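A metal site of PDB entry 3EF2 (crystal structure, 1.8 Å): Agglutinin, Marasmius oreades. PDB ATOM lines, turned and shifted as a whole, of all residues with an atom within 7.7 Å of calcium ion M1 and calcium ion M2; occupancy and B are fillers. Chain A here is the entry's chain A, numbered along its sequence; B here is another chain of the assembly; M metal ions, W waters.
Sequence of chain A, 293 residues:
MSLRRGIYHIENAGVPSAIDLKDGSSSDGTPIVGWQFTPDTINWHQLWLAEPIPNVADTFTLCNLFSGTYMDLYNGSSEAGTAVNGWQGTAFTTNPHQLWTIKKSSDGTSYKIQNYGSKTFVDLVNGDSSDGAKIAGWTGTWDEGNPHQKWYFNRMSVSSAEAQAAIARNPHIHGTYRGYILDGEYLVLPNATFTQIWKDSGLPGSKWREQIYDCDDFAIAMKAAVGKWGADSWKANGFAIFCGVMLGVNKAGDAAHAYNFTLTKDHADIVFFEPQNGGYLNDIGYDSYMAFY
The chain-end carboxylate of Tyr 293 lies within hydrogen-bond range of the backbone NH of Leu 182 (2.7 Å).
The side-chain hydroxyl of Tyr 186 is in hydrogen-bond range of the backbone NH of Asp 183, 3.0 Å away.
The backbone carbonyl oxygen (O) of Arg 209 of chain B is in hydrogen-bond range of the backbone NH (N) of Asp 214 of chain B.
The side-chain amide oxygen (OE1) of Gln 211 of chain B sits at hydrogen-bond distance from the backbone NH (N) of Gly 184 (2.8 Å).
The nearest printed residue that does not touch calcium ion M1 is Gln 211 of chain B (4.8 Å).
Of the 24 residues printed, 5 come within 4 Å of calcium ion M2.
The nearest printed residue that does not touch calcium ion M2 is Ala 240 (4.4 Å).
Calcium ion M1 is bound by O of Leu 182, water W1, OD1 of Asp 183, water W3, OD2 of Asp 214 of chain B and OD1 of Asp 216 of chain B.
Calcium ion M1 has six donor atoms within binding distance.
Slightly farther from calcium ion M1 lies OD1 of Asp 214 of chain B (3.1 Å).
Calcium ion M2 is bound by OD1 of Asp 214 of chain B, OD2 of Asp 216 of chain B, OD2 of Asp 183, OD2 of Asp 217 of chain B, water W2, O of Gln 211 of chain B, OD1 of Asp 183 and OD1 of Asp 216 of chain B.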
ATOM      1  N   ILE A 181       8.606 -30.577  -1.992  1.00  0.00           N
ATOM      2  CA  ILE A 181       9.399 -30.644  -3.212  1.00  0.00           C
ATOM      3  C   ILE A 181       9.835 -29.232  -3.608  1.00  0.00           C
ATOM      4  O   ILE A 181       9.003 -28.312  -3.677  1.00  0.00           O
ATOM      5  CB  ILE A 181       8.579 -31.289  -4.343  1.00  0.00           C
ATOM      6  CG1 ILE A 181       8.208 -32.733  -3.937  1.00  0.00           C
ATOM      7  CG2 ILE A 181       9.336 -31.211  -5.698  1.00  0.00           C
ATOM      8  CD1 ILE A 181       7.286 -33.481  -4.907  1.00  0.00           C
ATOM      9  N   LEU A 182      11.125 -29.091  -3.947  1.00  0.00           N
ATOM     10  CA  LEU A 182      11.701 -27.766  -4.163  1.00  0.00           C
ATOM     11  C   LEU A 182      12.043 -27.451  -5.625  1.00  0.00           C
ATOM     12  O   LEU A 182      12.091 -26.276  -6.024  1.00  0.00           O
ATOM     13  CB  LEU A 182      12.943 -27.586  -3.272  1.00  0.00           C
ATOM     14  CG  LEU A 182      12.768 -27.808  -1.759  1.00  0.00           C
ATOM     15  CD1 LEU A 182      14.138 -27.747  -1.090  1.00  0.00           C
ATOM     16  CD2 LEU A 182      11.855 -26.752  -1.147  1.00  0.00           C
ATOM     17  N   ASP A 183      12.285 -28.491  -6.431  1.00  0.00           N
ATOM     18  CA  ASP A 183      12.645 -28.297  -7.832  1.00  0.00           C
ATOM     19  C   ASP A 183      11.933 -29.347  -8.711  1.00  0.00           C
ATOM     20  O   ASP A 183      11.028 -30.031  -8.230  1.00  0.00           O
ATOM     21  CB  ASP A 183      14.184 -28.325  -8.013  1.00  0.00           C
ATOM     22  CG  ASP A 183      14.907 -27.144  -7.278  1.00  0.00           C
ATOM     23  OD1 ASP A 183      14.688 -25.955  -7.570  1.00  0.00           O
ATOM     24  OD2 ASP A 183      15.745 -27.407  -6.394  1.00  0.00           O
ATOM     25  N   GLY A 184      12.314 -29.475  -9.977  1.00  0.00           N
ATOM     26  CA  GLY A 184      11.522 -30.288 -10.929  1.00  0.00           C
ATOM     27  C   GLY A 184      12.279 -31.452 -11.552  1.00  0.00           C
ATOM     28  O   GLY A 184      11.679 -32.471 -11.923  1.00  0.00           O
ATOM     29  N   TYR A 186      16.345 -33.417 -11.373  1.00  0.00           N
ATOM     30  CA  TYR A 186      17.553 -33.509 -10.551  1.00  0.00           C
ATOM     31  C   TYR A 186      18.643 -34.438 -11.112  1.00  0.00           C
ATOM     32  O   TYR A 186      18.385 -35.618 -11.332  1.00  0.00           O
ATOM     33  CB  TYR A 186      17.206 -34.063  -9.168  1.00  0.00           C
ATOM     34  CG  TYR A 186      16.190 -33.287  -8.370  1.00  0.00           C
ATOM     35  CD1 TYR A 186      16.600 -32.309  -7.463  1.00  0.00           C
ATOM     36  CD2 TYR A 186      14.819 -33.536  -8.499  1.00  0.00           C
ATOM     37  CE1 TYR A 186      15.680 -31.604  -6.684  1.00  0.00           C
ATOM     38  CE2 TYR A 186      13.869 -32.840  -7.731  1.00  0.00           C
ATOM     39  CZ  TYR A 186      14.316 -31.878  -6.830  1.00  0.00           C
ATOM     40  OH  TYR A 186      13.413 -31.197  -6.056  1.00  0.00           O
ATOM     41  N   LYS A 223      23.009 -30.142   2.641  1.00  0.00           N
ATOM     42  CA  LYS A 223      22.136 -29.708   1.537  1.00  0.00           C
ATOM     43  C   LYS A 223      22.664 -28.405   0.919  1.00  0.00           C
ATOM     44  O   LYS A 223      22.682 -28.265  -0.316  1.00  0.00           O
ATOM     45  CB  LYS A 223      20.671 -29.549   1.959  1.00  0.00           C
ATOM     46  CG  LYS A 223      19.759 -29.276   0.721  1.00  0.00           C
ATOM     47  CD  LYS A 223      18.339 -29.804   0.863  1.00  0.00           C
ATOM     48  CE  LYS A 223      17.465 -29.380  -0.350  1.00  0.00           C
ATOM     49  NZ  LYS A 223      18.040 -29.754  -1.662  1.00  0.00           N
ATOM     50  N   GLY A 227      24.011 -27.758  -2.962  1.00  0.00           N
ATOM     51  CA  GLY A 227      23.449 -26.639  -3.749  1.00  0.00           C
ATOM     52  C   GLY A 227      24.550 -25.706  -4.288  1.00  0.00           C
ATOM     53  O   GLY A 227      24.513 -25.321  -5.470  1.00  0.00           O
ATOM     54  N   PHE A 239      17.751 -27.367 -13.961  1.00  0.00           N
ATOM     55  CA  PHE A 239      17.841 -28.613 -13.200  1.00  0.00           C
ATOM     56  C   PHE A 239      18.505 -28.299 -11.851  1.00  0.00           C
ATOM     57  O   PHE A 239      19.159 -27.239 -11.687  1.00  0.00           O
ATOM     58  CB  PHE A 239      18.670 -29.671 -13.965  1.00  0.00           C
ATOM     59  CG  PHE A 239      20.139 -29.316 -14.024  1.00  0.00           C
ATOM     60  CD1 PHE A 239      20.586 -28.312 -14.878  1.00  0.00           C
ATOM     61  CD2 PHE A 239      21.050 -29.928 -13.160  1.00  0.00           C
ATOM     62  CE1 PHE A 239      21.948 -27.937 -14.891  1.00  0.00           C
ATOM     63  CE2 PHE A 239      22.416 -29.567 -13.174  1.00  0.00           C
ATOM     64  CZ  PHE A 239      22.858 -28.572 -14.020  1.00  0.00           C
ATOM     65  N   ALA A 240      18.331 -29.225 -10.906  1.00  0.00           N
ATOM     66  CA  ALA A 240      19.002 -29.136  -9.594  1.00  0.00           C
ATOM     67  C   ALA A 240      19.819 -30.410  -9.344  1.00  0.00           C
ATOM     68  O   ALA A 240      19.805 -31.330 -10.168  1.00  0.00           O
ATOM     69  CB  ALA A 240      17.957 -28.929  -8.469  1.00  0.00           C
ATOM     70  N   ILE A 241      20.566 -30.437  -8.238  1.00  0.00           N
ATOM     71  CA  ILE A 241      21.332 -31.631  -7.853  1.00  0.00           C
ATOM     72  C   ILE A 241      20.551 -32.338  -6.755  1.00  0.00           C
ATOM     73  O   ILE A 241      20.099 -31.688  -5.804  1.00  0.00           O
ATOM     74  CB  ILE A 241      22.760 -31.266  -7.332  1.00  0.00           C
ATOM     75  CG1 ILE A 241      23.496 -30.265  -8.260  1.00  0.00           C
ATOM     76  CG2 ILE A 241      23.599 -32.553  -7.108  1.00  0.00           C
ATOM     77  CD1 ILE A 241      23.534 -30.665  -9.755  1.00  0.00           C
ATOM     78  N   TYR A 293      13.512 -31.574  -0.515  1.00  0.00           N
ATOM     79  CA  TYR A 293      14.456 -31.956  -1.563  1.00  0.00           C
ATOM     80  C   TYR A 293      14.058 -31.283  -2.885  1.00  0.00           C
ATOM     81  O   TYR A 293      14.904 -31.089  -3.767  1.00  0.00           O
ATOM     82  CB  TYR A 293      14.468 -33.484  -1.762  1.00  0.00           C
ATOM     83  CG  TYR A 293      13.112 -34.110  -2.089  1.00  0.00           C
ATOM     84  CD1 TYR A 293      12.261 -34.540  -1.056  1.00  0.00           C
ATOM     85  CD2 TYR A 293      12.697 -34.295  -3.405  1.00  0.00           C
ATOM     86  CE1 TYR A 293      11.016 -35.128  -1.334  1.00  0.00           C
ATOM     87  CE2 TYR A 293      11.452 -34.888  -3.704  1.00  0.00           C
ATOM     88  CZ  TYR A 293      10.630 -35.310  -2.661  1.00  0.00           C
ATOM     89  OH  TYR A 293       9.408 -35.898  -2.935  1.00  0.00           O
ATOM     90  OXT TYR A 293      12.902 -30.975  -3.099  1.00  0.00           O
ATOM     91  N   TRP B 208      20.478 -15.504  -9.313  1.00  0.00           N
ATOM     92  CA  TRP B 208      19.312 -16.383  -9.434  1.00  0.00           C
ATOM     93  C   TRP B 208      19.410 -17.173 -10.748  1.00  0.00           C
ATOM     94  O   TRP B 208      19.599 -16.593 -11.824  1.00  0.00           O
ATOM     95  CB  TRP B 208      17.988 -15.574  -9.403  1.00  0.00           C
ATOM     96  CG  TRP B 208      16.761 -16.457  -9.272  1.00  0.00           C
ATOM     97  CD1 TRP B 208      16.130 -16.794  -8.103  1.00  0.00           C
ATOM     98  CD2 TRP B 208      16.049 -17.135 -10.321  1.00  0.00           C
ATOM     99  NE1 TRP B 208      15.049 -17.606  -8.371  1.00  0.00           N
ATOM    100  CE2 TRP B 208      14.986 -17.839  -9.717  1.00  0.00           C
ATOM    101  CE3 TRP B 208      16.212 -17.207 -11.714  1.00  0.00           C
ATOM    102  CZ2 TRP B 208      14.071 -18.611 -10.460  1.00  0.00           C
ATOM    103  CZ3 TRP B 208      15.284 -17.975 -12.462  1.00  0.00           C
ATOM    104  CH2 TRP B 208      14.244 -18.668 -11.825  1.00  0.00           C
ATOM    105  N   ARG B 209      19.274 -18.497 -10.666  1.00  0.00           N
ATOM    106  CA  ARG B 209      19.347 -19.378 -11.845  1.00  0.00           C
ATOM    107  C   ARG B 209      18.300 -20.479 -11.720  1.00  0.00           C
ATOM    108  O   ARG B 209      18.193 -21.125 -10.682  1.00  0.00           O
ATOM    109  CB  ARG B 209      20.741 -20.020 -11.963  1.00  0.00           C
ATOM    110  CG  ARG B 209      21.890 -19.016 -12.203  1.00  0.00           C
ATOM    111  CD  ARG B 209      23.269 -19.699 -12.070  1.00  0.00           C
ATOM    112  NE  ARG B 209      23.387 -20.827 -12.992  1.00  0.00           N
ATOM    113  CZ  ARG B 209      24.344 -21.760 -12.973  1.00  0.00           C
ATOM    114  NH1 ARG B 209      25.295 -21.745 -12.054  1.00  0.00           N
ATOM    115  NH2 ARG B 209      24.318 -22.735 -13.869  1.00  0.00           N
ATOM    116  N   GLU B 210      17.549 -20.674 -12.790  1.00  0.00           N
ATOM    117  CA  GLU B 210      16.413 -21.600 -12.805  1.00  0.00           C
ATOM    118  C   GLU B 210      16.807 -22.985 -12.266  1.00  0.00           C
ATOM    119  O   GLU B 210      17.691 -23.627 -12.841  1.00  0.00           O
ATOM    120  CB  GLU B 210      15.912 -21.710 -14.246  1.00  0.00           C
ATOM    121  CG  GLU B 210      14.700 -22.573 -14.503  1.00  0.00           C
ATOM    122  CD  GLU B 210      14.541 -22.895 -15.997  1.00  0.00           C
ATOM    123  OE1 GLU B 210      15.065 -22.113 -16.842  1.00  0.00           O
ATOM    124  OE2 GLU B 210      13.947 -23.946 -16.328  1.00  0.00           O
ATOM    125  N   GLN B 211      16.154 -23.381 -11.169  1.00  0.00           N
ATOM    126  CA  GLN B 211      16.377 -24.643 -10.416  1.00  0.00           C
ATOM    127  C   GLN B 211      17.733 -24.845  -9.718  1.00  0.00           C
ATOM    128  O   GLN B 211      17.795 -25.285  -8.565  1.00  0.00           O
ATOM    129  CB  GLN B 211      16.026 -25.870 -11.270  1.00  0.00           C
ATOM    130  CG  GLN B 211      14.549 -25.882 -11.747  1.00  0.00           C
ATOM    131  CD  GLN B 211      14.084 -27.267 -12.191  1.00  0.00           C
ATOM    132  OE1 GLN B 211      14.304 -28.268 -11.507  1.00  0.00           O
ATOM    133  NE2 GLN B 211      13.432 -27.322 -13.361  1.00  0.00           N
ATOM    134  N   ILE B 212      18.813 -24.524 -10.450  1.00  0.00           N
ATOM    135  CA  ILE B 212      20.186 -24.854 -10.021  1.00  0.00           C
ATOM    136  C   ILE B 212      20.666 -23.906  -8.911  1.00  0.00           C
ATOM    137  O   ILE B 212      21.478 -24.288  -8.052  1.00  0.00           O
ATOM    138  CB  ILE B 212      21.157 -24.892 -11.267  1.00  0.00           C
ATOM    139  CG1 ILE B 212      22.524 -25.550 -10.922  1.00  0.00           C
ATOM    140  CG2 ILE B 212      21.297 -23.513 -11.884  1.00  0.00           C
ATOM    141  CD1 ILE B 212      22.436 -27.075 -10.517  1.00  0.00           C
ATOM    142  N   TYR B 213      20.127 -22.691  -8.907  1.00  0.00           N
ATOM    143  CA  TYR B 213      20.360 -21.782  -7.760  1.00  0.00           C
ATOM    144  C   TYR B 213      19.238 -20.764  -7.676  1.00  0.00           C
ATOM    145  O   TYR B 213      19.417 -19.576  -8.017  1.00  0.00           O
ATOM    146  CB  TYR B 213      21.732 -21.127  -7.778  1.00  0.00           C
ATOM    147  CG  TYR B 213      22.264 -20.966  -6.374  1.00  0.00           C
ATOM    148  CD1 TYR B 213      22.107 -19.757  -5.692  1.00  0.00           C
ATOM    149  CD2 TYR B 213      22.849 -22.043  -5.696  1.00  0.00           C
ATOM    150  CE1 TYR B 213      22.544 -19.608  -4.382  1.00  0.00           C
ATOM    151  CE2 TYR B 213      23.317 -21.915  -4.377  1.00  0.00           C
ATOM    152  CZ  TYR B 213      23.166 -20.677  -3.730  1.00  0.00           C
ATOM    153  OH  TYR B 213      23.604 -20.528  -2.420  1.00  0.00           O
ATOM    154  N   ASP B 214      18.063 -21.256  -7.284  1.00  0.00           N
ATOM    155  CA  ASP B 214      16.840 -20.441  -7.283  1.00  0.00           C
ATOM    156  C   ASP B 214      16.377 -20.218  -5.833  1.00  0.00           C
ATOM    157  O   ASP B 214      17.199 -20.331  -4.930  1.00  0.00           O
ATOM    158  CB  ASP B 214      15.762 -21.027  -8.211  1.00  0.00           C
ATOM    159  CG  ASP B 214      15.254 -22.406  -7.787  1.00  0.00           C
ATOM    160  OD1 ASP B 214      15.935 -23.138  -7.038  1.00  0.00           O
ATOM    161  OD2 ASP B 214      14.139 -22.747  -8.221  1.00  0.00           O
ATOM    162  N   OCS B 215      15.101 -19.915  -5.619  1.00  0.00           N
ATOM    163  CA  OCS B 215      14.566 -19.499  -4.296  1.00  0.00           C
ATOM    164  CB  OCS B 215      13.011 -19.512  -4.331  1.00  0.00           C
ATOM    165  SG  OCS B 215      12.326 -18.659  -5.746  1.00  0.00           S
ATOM    166  C   OCS B 215      15.042 -20.416  -3.167  1.00  0.00           C
ATOM    167  O   OCS B 215      15.580 -19.961  -2.155  1.00  0.00           O
ATOM    168  OD1 OCS B 215      12.619 -19.353  -6.956  1.00  0.00           O
ATOM    169  OD2 OCS B 215      12.927 -17.382  -5.740  1.00  0.00           O
ATOM    170  OD3 OCS B 215      10.902 -18.552  -5.615  1.00  0.00           O
ATOM    171  N   ASP B 216      14.808 -21.712  -3.341  1.00  0.00           N
ATOM    172  CA  ASP B 216      15.123 -22.699  -2.319  1.00  0.00           C
ATOM    173  C   ASP B 216      16.607 -22.670  -1.907  1.00  0.00           C
ATOM    174  O   ASP B 216      16.948 -22.792  -0.727  1.00  0.00           O
ATOM    175  CB  ASP B 216      14.617 -24.108  -2.737  1.00  0.00           C
ATOM    176  CG  ASP B 216      15.238 -24.599  -4.078  1.00  0.00           C
ATOM    177  OD1 ASP B 216      14.672 -24.440  -5.177  1.00  0.00           O
ATOM    178  OD2 ASP B 216      16.326 -25.161  -4.057  1.00  0.00           O
ATOM    179  N   ASP B 217      17.490 -22.497  -2.882  1.00  0.00           N
ATOM    180  CA  ASP B 217      18.933 -22.514  -2.645  1.00  0.00           C
ATOM    181  C   ASP B 217      19.351 -21.307  -1.818  1.00  0.00           C
ATOM    182  O   ASP B 217      20.143 -21.442  -0.876  1.00  0.00           O
ATOM    183  CB  ASP B 217      19.675 -22.576  -3.993  1.00  0.00           C
ATOM    184  CG  ASP B 217      19.263 -23.815  -4.781  1.00  0.00           C
ATOM    185  OD1 ASP B 217      19.707 -24.899  -4.374  1.00  0.00           O
ATOM    186  OD2 ASP B 217      18.438 -23.712  -5.727  1.00  0.00           O
ATOM    187  N   PHE B 218      18.811 -20.129  -2.146  1.00  0.00           N
ATOM    188  CA  PHE B 218      19.117 -18.899  -1.378  1.00  0.00           C
ATOM    189  C   PHE B 218      18.672 -19.038   0.083  1.00  0.00           C
ATOM    190  O   PHE B 218      19.436 -18.717   1.015  1.00  0.00           O
ATOM    191  CB  PHE B 218      18.447 -17.682  -2.013  1.00  0.00           C
ATOM    192  CG  PHE B 218      19.196 -17.097  -3.185  1.00  0.00           C
ATOM    193  CD1 PHE B 218      20.059 -16.018  -2.995  1.00  0.00           C
ATOM    194  CD2 PHE B 218      18.986 -17.570  -4.487  1.00  0.00           C
ATOM    195  CE1 PHE B 218      20.760 -15.443  -4.074  1.00  0.00           C
ATOM    196  CE2 PHE B 218      19.649 -16.984  -5.581  1.00  0.00           C
ATOM    197  CZ  PHE B 218      20.541 -15.919  -5.375  1.00  0.00           C
ATOM    198  N   ILE B 220      17.945 -21.849   1.893  1.00  0.00           N
ATOM    199  CA  ILE B 220      18.689 -22.872   2.614  1.00  0.00           C
ATOM    200  C   ILE B 220      20.119 -22.390   2.899  1.00  0.00           C
ATOM    201  O   ILE B 220      20.647 -22.628   3.991  1.00  0.00           O
ATOM    202  CB  ILE B 220      18.636 -24.240   1.876  1.00  0.00           C
ATOM    203  CG1 ILE B 220      17.289 -24.919   2.176  1.00  0.00           C
ATOM    204  CG2 ILE B 220      19.819 -25.151   2.270  1.00  0.00           C
ATOM    205  CD1 ILE B 220      16.868 -25.995   1.178  1.00  0.00           C
ATOM    206  N   ALA B 258      10.437 -19.340  -1.861  1.00  0.00           N
ATOM    207  CA  ALA B 258      11.147 -19.780  -0.645  1.00  0.00           C
ATOM    208  C   ALA B 258      11.935 -18.592  -0.114  1.00  0.00           C
ATOM    209  O   ALA B 258      12.505 -17.819  -0.880  1.00  0.00           O
ATOM    210  CB  ALA B 258      12.067 -20.951  -0.944  1.00  0.00           C
HETATM  211 CA    CA M   1      13.087 -24.394  -6.917  1.00  0.00          CA
HETATM  212 CA    CA M   2      16.736 -25.240  -6.393  1.00  0.00          CA
HETATM  213  O   HOH W   1      11.646 -24.670  -8.715  1.00  0.00           O
HETATM  214  O   HOH W   2      18.473 -26.730  -5.715  1.00  0.00           O
HETATM  215  O   HOH W   3      12.063 -22.716  -5.659  1.00  0.00           O
